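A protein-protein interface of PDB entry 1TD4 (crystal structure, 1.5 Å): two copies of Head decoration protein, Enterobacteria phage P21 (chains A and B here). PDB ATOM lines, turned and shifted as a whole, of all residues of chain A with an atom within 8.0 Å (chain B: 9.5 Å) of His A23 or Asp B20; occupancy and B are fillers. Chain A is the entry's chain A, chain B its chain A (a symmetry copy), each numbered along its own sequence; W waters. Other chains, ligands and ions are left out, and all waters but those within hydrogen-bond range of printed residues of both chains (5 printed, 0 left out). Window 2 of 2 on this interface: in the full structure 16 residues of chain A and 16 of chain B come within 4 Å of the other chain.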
ATOM      1  N   PHE A  16      32.149  29.223 -25.709  1.00  0.00           N
ATOM      2  CA  PHE A  16      31.223  28.116 -25.980  1.00  0.00           C
ATOM      3  C   PHE A  16      31.496  27.394 -27.296  1.00  0.00           C
ATOM      4  O   PHE A  16      31.951  27.990 -28.256  1.00  0.00           O
ATOM      5  CB  PHE A  16      29.775  28.623 -26.004  1.00  0.00           C
ATOM      6  CG  PHE A  16      29.424  29.432 -24.759  1.00  0.00           C
ATOM      7  CD1 PHE A  16      29.044  28.787 -23.593  1.00  0.00           C
ATOM      8  CD2 PHE A  16      29.466  30.816 -24.777  1.00  0.00           C
ATOM      9  CE1 PHE A  16      28.712  29.496 -22.444  1.00  0.00           C
ATOM     10  CE2 PHE A  16      29.125  31.533 -23.642  1.00  0.00           C
ATOM     11  CZ  PHE A  16      28.728  30.879 -22.485  1.00  0.00           C
ATOM     12  N   ASP A  20      23.452  25.183 -27.030  1.00  0.00           N
ATOM     13  CA  ASP A  20      22.510  24.910 -25.958  1.00  0.00           C
ATOM     14  C   ASP A  20      22.686  25.940 -24.862  1.00  0.00           C
ATOM     15  O   ASP A  20      23.787  26.360 -24.517  1.00  0.00           O
ATOM     16  CB  ASP A  20      22.681  23.497 -25.396  1.00  0.00           C
ATOM     17  CG  ASP A  20      24.087  23.048 -25.064  1.00  0.00           C
ATOM     18  OD1 ASP A  20      24.994  23.127 -25.921  1.00  0.00           O
ATOM     19  OD2 ASP A  20      24.343  22.554 -23.929  1.00  0.00           O
ATOM     20  N   PRO A  21      21.569  26.402 -24.330  1.00  0.00           N
ATOM     21  CA  PRO A  21      21.639  27.476 -23.319  1.00  0.00           C
ATOM     22  C   PRO A  21      22.552  27.145 -22.153  1.00  0.00           C
ATOM     23  O   PRO A  21      22.535  26.013 -21.648  1.00  0.00           O
ATOM     24  CB  PRO A  21      20.204  27.536 -22.808  1.00  0.00           C
ATOM     25  CG  PRO A  21      19.406  27.132 -24.004  1.00  0.00           C
ATOM     26  CD  PRO A  21      20.195  26.014 -24.655  1.00  0.00           C
ATOM     27  N   ALA A  22      23.340  28.146 -21.788  1.00  0.00           N
ATOM     28  CA  ALA A  22      24.251  27.997 -20.663  1.00  0.00           C
ATOM     29  C   ALA A  22      23.654  28.691 -19.437  1.00  0.00           C
ATOM     30  O   ALA A  22      23.848  29.886 -19.220  1.00  0.00           O
ATOM     31  CB  ALA A  22      25.625  28.546 -21.049  1.00  0.00           C
ATOM     32  N   HIS A  23      22.911  27.914 -18.634  1.00  0.00           N
ATOM     33  CA  HIS A  23      22.265  28.467 -17.463  1.00  0.00           C
ATOM     34  C   HIS A  23      23.243  28.577 -16.286  1.00  0.00           C
ATOM     35  O   HIS A  23      24.131  27.741 -16.240  1.00  0.00           O
ATOM     36  CB  HIS A  23      21.100  27.577 -16.981  1.00  0.00           C
ATOM     37  CG  HIS A  23      20.064  27.458 -18.083  1.00  0.00           C
ATOM     38  ND1 HIS A  23      19.534  26.258 -18.468  1.00  0.00           N
ATOM     39  CD2 HIS A  23      19.513  28.404 -18.884  1.00  0.00           C
ATOM     40  CE1 HIS A  23      18.662  26.486 -19.455  1.00  0.00           C
ATOM     41  NE2 HIS A  23      18.624  27.782 -19.731  1.00  0.00           N
ATOM     42  N   THR A  24      23.020  29.539 -15.404  1.00  0.00           N
ATOM     43  CA  THR A  24      23.852  29.683 -14.213  1.00  0.00           C
ATOM     44  C   THR A  24      23.085  29.372 -12.940  1.00  0.00           C
ATOM     45  O   THR A  24      21.839  29.332 -12.917  1.00  0.00           O
ATOM     46  CB  THR A  24      24.431  31.095 -14.099  1.00  0.00           C
ATOM     47  OG1 THR A  24      23.325  32.011 -13.923  1.00  0.00           O
ATOM     48  CG2 THR A  24      25.161  31.537 -15.353  1.00  0.00           C
ATOM     49  N   ALA A  25      23.836  29.128 -11.866  1.00  0.00           N
ATOM     50  CA  ALA A  25      23.260  28.780 -10.566  1.00  0.00           C
ATOM     51  C   ALA A  25      24.153  29.372  -9.472  1.00  0.00           C
ATOM     52  O   ALA A  25      25.289  29.707  -9.763  1.00  0.00           O
ATOM     53  CB  ALA A  25      23.179  27.270 -10.368  1.00  0.00           C
ATOM     54  N   ILE A  64      30.939  25.068 -13.627  1.00  0.00           N
ATOM     55  CA  ILE A  64      32.072  25.846 -14.099  1.00  0.00           C
ATOM     56  C   ILE A  64      31.926  27.266 -13.579  1.00  0.00           C
ATOM     57  O   ILE A  64      30.926  27.950 -13.788  1.00  0.00           O
ATOM     58  CB  ILE A  64      32.130  25.878 -15.638  1.00  0.00           C
ATOM     59  CG1 ILE A  64      32.400  24.514 -16.242  1.00  0.00           C
ATOM     60  CG2 ILE A  64      33.117  26.962 -16.118  1.00  0.00           C
ATOM     61  CD1 ILE A  64      32.275  24.464 -17.753  1.00  0.00           C
ATOM     62  N   VAL A  66      31.589  31.081 -13.049  1.00  0.00           N
ATOM     63  CA  VAL A  66      31.222  32.166 -13.950  1.00  0.00           C
ATOM     64  C   VAL A  66      32.018  33.448 -13.641  1.00  0.00           C
ATOM     65  O   VAL A  66      32.485  34.069 -14.578  1.00  0.00           O
ATOM     66  CB  VAL A  66      29.750  32.586 -13.871  1.00  0.00           C
ATOM     67  CG1 VAL A  66      29.421  33.730 -14.828  1.00  0.00           C
ATOM     68  CG2 VAL A  66      28.846  31.389 -14.189  1.00  0.00           C
ATOM     69  N   THR A  77      28.867  31.829  -8.222  1.00  0.00           N
ATOM     70  CA  THR A  77      27.983  31.614  -9.353  1.00  0.00           C
ATOM     71  C   THR A  77      28.665  30.663 -10.325  1.00  0.00           C
ATOM     72  O   THR A  77      29.856  30.907 -10.599  1.00  0.00           O
ATOM     73  CB  THR A  77      27.654  32.965 -10.027  1.00  0.00           C
ATOM     74  OG1 THR A  77      26.973  33.790  -9.073  1.00  0.00           O
ATOM     75  CG2 THR A  77      26.709  32.800 -11.202  1.00  0.00           C
ATOM     76  N   TYR A  78      27.916  29.656 -10.761  1.00  0.00           N
ATOM     77  CA  TYR A  78      28.489  28.681 -11.696  1.00  0.00           C
ATOM     78  C   TYR A  78      27.535  28.366 -12.840  1.00  0.00           C
ATOM     79  O   TYR A  78      26.336  28.468 -12.747  1.00  0.00           O
ATOM     80  CB  TYR A  78      28.866  27.408 -10.971  1.00  0.00           C
ATOM     81  CG  TYR A  78      27.813  26.612 -10.238  1.00  0.00           C
ATOM     82  CD1 TYR A  78      27.355  26.960  -8.981  1.00  0.00           C
ATOM     83  CD2 TYR A  78      27.283  25.466 -10.824  1.00  0.00           C
ATOM     84  CE1 TYR A  78      26.388  26.204  -8.328  1.00  0.00           C
ATOM     85  CE2 TYR A  78      26.320  24.696 -10.185  1.00  0.00           C
ATOM     86  CZ  TYR A  78      25.874  25.079  -8.928  1.00  0.00           C
ATOM     87  OH  TYR A  78      24.927  24.306  -8.293  1.00  0.00           O
ATOM     88  N   TYR A  79      28.099  27.959 -13.966  1.00  0.00           N
ATOM     89  CA  TYR A  79      27.301  27.409 -15.052  1.00  0.00           C
ATOM     90  C   TYR A  79      26.828  26.006 -14.670  1.00  0.00           C
ATOM     91  O   TYR A  79      27.698  25.216 -14.238  1.00  0.00           O
ATOM     92  CB  TYR A  79      28.116  27.333 -16.340  1.00  0.00           C
ATOM     93  CG  TYR A  79      28.475  28.674 -16.937  1.00  0.00           C
ATOM     94  CD1 TYR A  79      29.784  29.140 -16.953  1.00  0.00           C
ATOM     95  CD2 TYR A  79      27.507  29.501 -17.497  1.00  0.00           C
ATOM     96  CE1 TYR A  79      30.142  30.359 -17.497  1.00  0.00           C
ATOM     97  CE2 TYR A  79      27.865  30.729 -18.046  1.00  0.00           C
ATOM     98  CZ  TYR A  79      29.171  31.164 -18.046  1.00  0.00           C
ATOM     99  OH  TYR A  79      29.535  32.374 -18.580  1.00  0.00           O
ATOM    100  N   LYS A  80      25.549  25.751 -14.884  1.00  0.00           N
ATOM    101  CA  LYS A  80      24.997  24.426 -14.604  1.00  0.00           C
ATOM    102  C   LYS A  80      24.602  23.775 -15.939  1.00  0.00           C
ATOM    103  O   LYS A  80      24.177  22.624 -15.962  1.00  0.00           O
ATOM    104  CB  LYS A  80      23.824  24.435 -13.632  1.00  0.00           C
ATOM    105  CG  LYS A  80      22.619  25.271 -14.086  1.00  0.00           C
ATOM    106  CD  LYS A  80      21.380  24.941 -13.271  1.00  0.00           C
ATOM    107  CE  LYS A  80      20.141  25.646 -13.810  1.00  0.00           C
ATOM    108  NZ  LYS A  80      18.910  25.341 -12.989  1.00  0.00           N
ATOM    109  N   SER A  81      24.735  24.482 -17.052  1.00  0.00           N
ATOM    110  CA  SER A  81      24.478  23.860 -18.348  1.00  0.00           C
ATOM    111  C   SER A  81      25.302  24.568 -19.427  1.00  0.00           C
ATOM    112  O   SER A  81      25.912  25.603 -19.129  1.00  0.00           O
ATOM    113  CB  SER A  81      23.001  23.876 -18.748  1.00  0.00           C
ATOM    114  OG  SER A  81      22.594  25.218 -19.042  1.00  0.00           O
ATOM    115  N   GLY A  82      25.266  23.987 -20.631  1.00  0.00           N
ATOM    116  CA  GLY A  82      25.961  24.541 -21.766  1.00  0.00           C
ATOM    117  C   GLY A  82      27.057  23.624 -22.319  1.00  0.00           C
ATOM    118  O   GLY A  82      27.441  22.629 -21.673  1.00  0.00           O
ATOM    119  N   THR A  83      27.565  23.975 -23.502  1.00  0.00           N
ATOM    120  CA  THR A  83      28.657  23.270 -24.149  1.00  0.00           C
ATOM    121  C   THR A  83      29.850  24.220 -24.271  1.00  0.00           C
ATOM    122  O   THR A  83      29.690  25.224 -24.993  1.00  0.00           O
ATOM    123  CB  THR A  83      28.284  22.798 -25.566  1.00  0.00           C
ATOM    124  OG1 THR A  83      27.162  21.925 -25.432  1.00  0.00           O
ATOM    125  CG2 THR A  83      29.450  22.043 -26.193  1.00  0.00           C
ATOM    126  N   PHE A  84      30.929  23.952 -23.563  1.00  0.00           N
ATOM    127  CA  PHE A  84      32.066  24.877 -23.492  1.00  0.00           C
ATOM    128  C   PHE A  84      33.200  24.513 -24.419  1.00  0.00           C
ATOM    129  O   PHE A  84      33.348  23.331 -24.766  1.00  0.00           O
ATOM    130  CB  PHE A  84      32.574  24.907 -22.024  1.00  0.00           C
ATOM    131  CG  PHE A  84      31.552  25.666 -21.165  1.00  0.00           C
ATOM    132  CD1 PHE A  84      30.370  25.053 -20.792  1.00  0.00           C
ATOM    133  CD2 PHE A  84      31.789  26.966 -20.783  1.00  0.00           C
ATOM    134  CE1 PHE A  84      29.424  25.729 -20.058  1.00  0.00           C
ATOM    135  CE2 PHE A  84      30.851  27.652 -20.036  1.00  0.00           C
ATOM    136  CZ  PHE A  84      29.654  27.040 -19.685  1.00  0.00           C
ATOM    137  N   ALA A 108      24.447  18.693 -16.853  1.00  0.00           N
ATOM    138  CA  ALA A 108      23.982  19.240 -18.132  1.00  0.00           C
ATOM    139  C   ALA A 108      25.103  19.952 -18.886  1.00  0.00           C
ATOM    140  O   ALA A 108      24.812  20.479 -19.969  1.00  0.00           O
ATOM    141  CB  ALA A 108      22.802  20.183 -17.931  1.00  0.00           C
ATOM    142  N   LEU A 109      26.326  19.935 -18.323  1.00  0.00           N
ATOM    143  CA  LEU A 109      27.479  20.562 -18.941  1.00  0.00           C
ATOM    144  C   LEU A 109      28.232  19.581 -19.843  1.00  0.00           C
ATOM    145  O   LEU A 109      28.224  18.376 -19.555  1.00  0.00           O
ATOM    146  CB  LEU A 109      28.508  21.055 -17.917  1.00  0.00           C
ATOM    147  CG  LEU A 109      27.950  22.094 -16.937  1.00  0.00           C
ATOM    148  CD1 LEU A 109      28.656  21.958 -15.582  1.00  0.00           C
ATOM    149  CD2 LEU A 109      28.138  23.481 -17.517  1.00  0.00           C
ATOM    150  N   PHE B  16       9.334  29.510  -8.623  1.00  0.00           N
ATOM    151  CA  PHE B  16      10.590  29.614  -9.376  1.00  0.00           C
ATOM    152  C   PHE B  16      11.335  30.927  -9.151  1.00  0.00           C
ATOM    153  O   PHE B  16      10.731  31.960  -8.924  1.00  0.00           O
ATOM    154  CB  PHE B  16      10.325  29.468 -10.881  1.00  0.00           C
ATOM    155  CG  PHE B  16       9.510  28.219 -11.207  1.00  0.00           C
ATOM    156  CD1 PHE B  16      10.138  26.989 -11.326  1.00  0.00           C
ATOM    157  CD2 PHE B  16       8.142  28.295 -11.400  1.00  0.00           C
ATOM    158  CE1 PHE B  16       9.425  25.835 -11.628  1.00  0.00           C
ATOM    159  CE2 PHE B  16       7.423  27.154 -11.714  1.00  0.00           C
ATOM    160  CZ  PHE B  16       8.063  25.930 -11.850  1.00  0.00           C
ATOM    161  N   ALA B  17      12.657  30.871  -9.218  1.00  0.00           N
ATOM    162  CA  ALA B  17      13.539  31.995  -9.017  1.00  0.00           C
ATOM    163  C   ALA B  17      14.432  32.193 -10.242  1.00  0.00           C
ATOM    164  O   ALA B  17      15.517  32.752 -10.164  1.00  0.00           O
ATOM    165  CB  ALA B  17      14.389  31.776  -7.762  1.00  0.00           C
ATOM    166  N   GLY B  18      13.976  31.735 -11.396  1.00  0.00           N
ATOM    167  CA  GLY B  18      14.721  31.857 -12.648  1.00  0.00           C
ATOM    168  C   GLY B  18      13.828  31.376 -13.796  1.00  0.00           C
ATOM    169  O   GLY B  18      12.829  30.672 -13.520  1.00  0.00           O
ATOM    170  N   ASN B  19      14.206  31.787 -15.012  1.00  0.00           N
ATOM    171  CA  ASN B  19      13.407  31.515 -16.189  1.00  0.00           C
ATOM    172  C   ASN B  19      13.747  30.257 -16.981  1.00  0.00           C
ATOM    173  O   ASN B  19      13.051  29.954 -17.962  1.00  0.00           O
ATOM    174  CB  ASN B  19      13.562  32.701 -17.181  1.00  0.00           C
ATOM    175  CG  ASN B  19      15.021  33.156 -17.142  1.00  0.00           C
ATOM    176  OD1 ASN B  19      15.333  34.179 -16.526  1.00  0.00           O
ATOM    177  ND2 ASN B  19      15.877  32.366 -17.777  1.00  0.00           N
ATOM    178  N   ASP B  20      14.795  29.522 -16.615  1.00  0.00           N
ATOM    179  CA  ASP B  20      15.152  28.326 -17.359  1.00  0.00           C
ATOM    180  C   ASP B  20      14.044  27.303 -17.225  1.00  0.00           C
ATOM    181  O   ASP B  20      13.432  27.122 -16.176  1.00  0.00           O
ATOM    182  CB  ASP B  20      16.483  27.738 -16.886  1.00  0.00           C
ATOM    183  CG  ASP B  20      16.680  27.577 -15.395  1.00  0.00           C
ATOM    184  OD1 ASP B  20      16.506  28.548 -14.626  1.00  0.00           O
ATOM    185  OD2 ASP B  20      17.057  26.467 -14.921  1.00  0.00           O
ATOM    186  N   PRO B  21      13.738  26.647 -18.329  1.00  0.00           N
ATOM    187  CA  PRO B  21      12.609  25.696 -18.316  1.00  0.00           C
ATOM    188  C   PRO B  21      12.718  24.648 -17.224  1.00  0.00           C
ATOM    189  O   PRO B  21      13.806  24.102 -16.989  1.00  0.00           O
ATOM    190  CB  PRO B  21      12.751  25.004 -19.666  1.00  0.00           C
ATOM    191  CG  PRO B  21      13.348  26.068 -20.527  1.00  0.00           C
ATOM    192  CD  PRO B  21      14.361  26.774 -19.647  1.00  0.00           C
ATOM    193  N   ALA B  22      11.583  24.429 -16.576  1.00  0.00           N
ATOM    194  CA  ALA B  22      11.516  23.428 -15.522  1.00  0.00           C
ATOM    195  C   ALA B  22      10.857  22.162 -16.071  1.00  0.00           C
ATOM    196  O   ALA B  22       9.635  22.017 -16.055  1.00  0.00           O
ATOM    197  CB  ALA B  22      10.776  24.011 -14.318  1.00  0.00           C
ATOM    198  N   HIS B  23      11.694  21.238 -16.569  1.00  0.00           N
ATOM    199  CA  HIS B  23      11.184  20.014 -17.149  1.00  0.00           C
ATOM    200  C   HIS B  23      10.848  18.981 -16.066  1.00  0.00           C
ATOM    201  O   HIS B  23      11.525  19.021 -15.051  1.00  0.00           O
ATOM    202  CB  HIS B  23      12.220  19.351 -18.080  1.00  0.00           C
ATOM    203  CG  HIS B  23      12.569  20.302 -19.209  1.00  0.00           C
ATOM    204  ND1 HIS B  23      13.860  20.568 -19.574  1.00  0.00           N
ATOM    205  CD2 HIS B  23      11.774  21.059 -20.005  1.00  0.00           C
ATOM    206  CE1 HIS B  23      13.835  21.439 -20.587  1.00  0.00           C
ATOM    207  NE2 HIS B  23      12.581  21.757 -20.875  1.00  0.00           N
ATOM    208  N   TYR B  79      10.536  17.297 -10.927  1.00  0.00           N
ATOM    209  CA  TYR B  79      11.270  18.247 -11.749  1.00  0.00           C
ATOM    210  C   TYR B  79      12.707  17.754 -11.929  1.00  0.00           C
ATOM    211  O   TYR B  79      13.318  17.409 -10.893  1.00  0.00           O
ATOM    212  CB  TYR B  79      11.291  19.627 -11.097  1.00  0.00           C
ATOM    213  CG  TYR B  79       9.946  20.317 -11.045  1.00  0.00           C
ATOM    214  CD1 TYR B  79       9.277  20.522  -9.844  1.00  0.00           C
ATOM    215  CD2 TYR B  79       9.321  20.776 -12.199  1.00  0.00           C
ATOM    216  CE1 TYR B  79       8.052  21.155  -9.766  1.00  0.00           C
ATOM    217  CE2 TYR B  79       8.087  21.413 -12.122  1.00  0.00           C
ATOM    218  CZ  TYR B  79       7.447  21.602 -10.917  1.00  0.00           C
ATOM    219  OH  TYR B  79       6.229  22.225 -10.831  1.00  0.00           O
ATOM    220  N   LYS B  80      13.176  17.787 -13.164  1.00  0.00           N
ATOM    221  CA  LYS B  80      14.554  17.387 -13.447  1.00  0.00           C
ATOM    222  C   LYS B  80      15.338  18.633 -13.888  1.00  0.00           C
ATOM    223  O   LYS B  80      16.542  18.556 -14.114  1.00  0.00           O
ATOM    224  CB  LYS B  80      14.677  16.271 -14.476  1.00  0.00           C
ATOM    225  CG  LYS B  80      14.075  16.594 -15.850  1.00  0.00           C
ATOM    226  CD  LYS B  80      14.551  15.611 -16.906  1.00  0.00           C
ATOM    227  CE  LYS B  80      14.088  16.009 -18.303  1.00  0.00           C
ATOM    228  NZ  LYS B  80      14.539  15.023 -19.355  1.00  0.00           N
ATOM    229  N   SER B  81      14.686  19.779 -14.014  1.00  0.00           N
ATOM    230  CA  SER B  81      15.417  21.006 -14.321  1.00  0.00           C
ATOM    231  C   SER B  81      14.651  22.211 -13.766  1.00  0.00           C
ATOM    232  O   SER B  81      13.516  22.034 -13.307  1.00  0.00           O
ATOM    233  CB  SER B  81      15.664  21.209 -15.817  1.00  0.00           C
ATOM    234  OG  SER B  81      14.426  21.499 -16.477  1.00  0.00           O
ATOM    235  N   GLY B  82      15.302  23.376 -13.853  1.00  0.00           N
ATOM    236  CA  GLY B  82      14.711  24.613 -13.406  1.00  0.00           C
ATOM    237  C   GLY B  82      15.470  25.270 -12.249  1.00  0.00           C
ATOM    238  O   GLY B  82      16.350  24.642 -11.626  1.00  0.00           O
ATOM    239  N   THR B  83      15.112  26.522 -11.955  1.00  0.00           N
ATOM    240  CA  THR B  83      15.668  27.278 -10.849  1.00  0.00           C
ATOM    241  C   THR B  83      14.548  27.593  -9.857  1.00  0.00           C
ATOM    242  O   THR B  83      13.628  28.326 -10.271  1.00  0.00           O
ATOM    243  CB  THR B  83      16.278  28.615 -11.309  1.00  0.00           C
ATOM    244  OG1 THR B  83      17.311  28.302 -12.243  1.00  0.00           O
ATOM    245  CG2 THR B  83      16.870  29.361 -10.119  1.00  0.00           C
ATOM    246  N   PHE B  84      14.596  27.023  -8.669  1.00  0.00           N
ATOM    247  CA  PHE B  84      13.497  27.137  -7.703  1.00  0.00           C
ATOM    248  C   PHE B  84      13.728  28.191  -6.647  1.00  0.00           C
ATOM    249  O   PHE B  84      14.888  28.508  -6.346  1.00  0.00           O
ATOM    250  CB  PHE B  84      13.299  25.750  -7.030  1.00  0.00           C
ATOM    251  CG  PHE B  84      12.664  24.794  -8.051  1.00  0.00           C
ATOM    252  CD1 PHE B  84      13.437  24.247  -9.058  1.00  0.00           C
ATOM    253  CD2 PHE B  84      11.323  24.497  -7.990  1.00  0.00           C
ATOM    254  CE1 PHE B  84      12.880  23.421 -10.007  1.00  0.00           C
ATOM    255  CE2 PHE B  84      10.755  23.661  -8.931  1.00  0.00           C
ATOM    256  CZ  PHE B  84      11.529  23.131  -9.956  1.00  0.00           C
ATOM    257  N   ALA B  85      12.651  28.745  -6.078  1.00  0.00           N
ATOM    258  CA  ALA B  85      12.786  29.646  -4.944  1.00  0.00           C
ATOM    259  C   ALA B  85      13.067  28.806  -3.701  1.00  0.00           C
ATOM    260  O   ALA B  85      12.300  27.891  -3.399  1.00  0.00           O
ATOM    261  CB  ALA B  85      11.553  30.496  -4.719  1.00  0.00           C
ATOM    262  N   SER B 107      23.108  18.284 -11.000  1.00  0.00           N
ATOM    263  CA  SER B 107      21.880  18.044 -11.782  1.00  0.00           C
ATOM    264  C   SER B 107      21.540  19.293 -12.590  1.00  0.00           C
ATOM    265  O   SER B 107      22.310  20.258 -12.510  1.00  0.00           O
ATOM    266  CB  SER B 107      20.705  17.702 -10.851  1.00  0.00           C
ATOM    267  OG  SER B 107      20.277  18.898 -10.191  1.00  0.00           O
ATOM    268  N   ALA B 108      20.425  19.324 -13.301  1.00  0.00           N
ATOM    269  CA  ALA B 108      20.036  20.551 -14.005  1.00  0.00           C
ATOM    270  C   ALA B 108      19.198  21.472 -13.121  1.00  0.00           C
ATOM    271  O   ALA B 108      18.791  22.527 -13.628  1.00  0.00           O
ATOM    272  CB  ALA B 108      19.286  20.233 -15.292  1.00  0.00           C
ATOM    273  N   LEU B 109      18.985  21.074 -11.853  1.00  0.00           N
ATOM    274  CA  LEU B 109      18.218  21.862 -10.906  1.00  0.00           C
ATOM    275  C   LEU B 109      19.116  22.817 -10.116  1.00  0.00           C
ATOM    276  O   LEU B 109      20.287  22.484  -9.886  1.00  0.00           O
ATOM    277  CB  LEU B 109      17.505  21.001  -9.856  1.00  0.00           C
ATOM    278  CG  LEU B 109      16.513  19.998 -10.455  1.00  0.00           C
ATOM    279  CD1 LEU B 109      16.453  18.742  -9.575  1.00  0.00           C
ATOM    280  CD2 LEU B 109      15.152  20.648 -10.576  1.00  0.00           C
ATOM    281  N   SER B 110      18.533  23.910  -9.654  1.00  0.00           N
ATOM    282  CA  SER B 110      19.222  24.816  -8.736  1.00  0.00           C
ATOM    283  C   SER B 110      18.138  25.579  -7.985  1.00  0.00           C
ATOM    284  O   SER B 110      16.952  25.453  -8.319  1.00  0.00           O
ATOM    285  CB  SER B 110      20.096  25.793  -9.476  1.00  0.00           C
ATOM    286  OG  SER B 110      19.379  26.431 -10.531  1.00  0.00           O
ATOM    287  N   HIS B 111      18.588  26.378  -7.015  1.00  0.00           N
ATOM    288  CA  HIS B 111      17.619  27.189  -6.283  1.00  0.00           C
ATOM    289  C   HIS B 111      18.318  28.436  -5.769  1.00  0.00           C
ATOM    290  O   HIS B 111      19.552  28.451  -5.633  1.00  0.00           O
ATOM    291  CB  HIS B 111      16.971  26.341  -5.179  1.00  0.00           C
ATOM    292  CG  HIS B 111      17.864  26.056  -4.005  1.00  0.00           C
ATOM    293  ND1 HIS B 111      17.901  26.809  -2.842  1.00  0.00           N
ATOM    294  CD2 HIS B 111      18.734  25.011  -3.831  1.00  0.00           C
ATOM    295  CE1 HIS B 111      18.763  26.275  -1.999  1.00  0.00           C
ATOM    296  NE2 HIS B 111      19.296  25.192  -2.582  1.00  0.00           N
ATOM    297  N   ALA B 112      17.476  29.426  -5.488  1.00  0.00           N
ATOM    298  CA  ALA B 112      18.019  30.717  -5.053  1.00  0.00           C
ATOM    299  C   ALA B 112      16.946  31.440  -4.238  1.00  0.00           C
ATOM    300  O   ALA B 112      15.756  31.166  -4.375  1.00  0.00           O
ATOM    301  CB  ALA B 112      18.484  31.561  -6.218  1.00  0.00           C
HETATM  302  O   HOH W   1      22.288  23.633  -8.162  1.00  0.00           O
HETATM  303  O   HOH W   2      19.376  28.841 -14.208  1.00  0.00           O
HETATM  304  O   HOH W   3      23.344  22.365 -10.590  1.00  0.00           O
HETATM  305  O   HOH W   4      24.283  20.349 -14.422  1.00  0.00           O
HETATM  306  O   HOH W   5      19.766  28.997 -11.241  1.00  0.00           O
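Printed residues of chain B that touch a printed residue of chain A: Asp B20, Gly B82, Thr B83, Ala B108, Leu B109 and Ser B110. Along chain B the printed residues that touch a printed residue of chain A span positions 20 to 110. Among the printed residues, 8 pairs touch across the chains. Among the printed residues, Asp or Glu carboxylates within 4 Å of a Lys or Arg side-chain nitrogen of the other chain: Lys A80 with Asp B20 (2.9 Å).
OG1 of Thr B83 is in hydrogen-bond range of NZ of Lys A80, 3.4 Å away. The side-chain amino group (NZ) of Lys A80 lies within hydrogen-bond range of the backbone carbonyl oxygen (O) of Ala B108, at 2.9 Å. NZ of Lys A80 is in salt-bridge range of OD2 of Asp B20 (2.9 Å). The side-chain amino group of Lys A80 sits at hydrogen-bond distance from the side-chain hydroxyl of Ser B110 (2.7 Å). The backbone carbonyl oxygen (O) of Gly B82 is in hydrogen-bond range of the side-chain amino group (NZ) of Lys A80, at 3.0 Å.
Lys A80 touches Asp B20, but with the chains exchanged Asp A20 does not touch Lys B80 (13.2 Å). Lys A80 touches Gly B82, but with the chains exchanged Gly A82 does not touch Lys B80 (12.2 Å). Lys A80 touches Ala B108, but with the chains exchanged Ala A108 does not touch Lys B80 (7.5 Å). Lys A80 touches Leu B109, but with the chains exchanged Leu A109 does not touch Lys B80 (10.7 Å). 13 positions are printed for both chains.
Printed residues of chain B within 4 Å of His A23: Asp B20 (3.6 Å). Of the printed residues of chain B, Ala A25 touches Ser B110. Lys A80 touches six residues of chain B. No residue of chain B comes within 4 Å of Ser A81. Gly B18 touches none of the printed residues of chain A. Of chain A, only His A23 (3.6 Å) and Lys A80 (2.9 Å) come within 4 Å of Asp B20. Of chain A, only Lys A80 (3.0 Å) comes within 4 Å of Gly B82. Of the printed residues of chain A, Thr B83 touches Lys A80 (3.4 Å). Ser B107 touches none of the printed residues of chain A. Printed residues of chain A within 4 Å of Ala B108: Lys A80. Of the printed residues of chain A, Ser B110 touches Ala A25 (3.5 Å) and Lys A80 (2.7 Å). The nearest residue of chain A that does not touch Asp B20 is Thr A24 (5.7 Å).
The side-chain carboxylate of Asp B20 lies within hydrogen-bond range of the side-chain hydroxyl of Thr B83. The backbone carbonyl oxygen (O) of Gly B82 lies within hydrogen-bond range of the backbone NH (N) of Ser B110, at 3.0 Å. N of His A23 sits at hydrogen-bond distance from OG of Ser A81 (2.7 Å). N of Ala B17 lies within hydrogen-bond range of O of Thr B83.
Water W5 lies within hydrogen-bond range of O of Thr A24, OG of Ser B110 and OG1 of Thr B83. Water W1 bridges OH of Tyr A78 (2.7 Å) and O of Leu B109 (2.9 Å). Water W4 lies within hydrogen-bond range of O of Ser B107 (2.7 Å), O of Lys A80 (2.7 Å) and N of Ala A108 (2.9 Å). Water W3 lies within hydrogen-bond range of the backbone carbonyl oxygen (O) of Ser B107 (3.0 Å), the backbone carbonyl oxygen (O) of Leu B109 (3.1 Å) and the side-chain hydroxyl (OH) of Tyr A78 (3.4 Å).
Among the printed residues, merely in contact across the chains: His A23 with Asp B20 (3.6 Å), Ala A25 with Ser B110 (3.5 Å) and Lys A80 with Leu B109 (3.8 Å).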
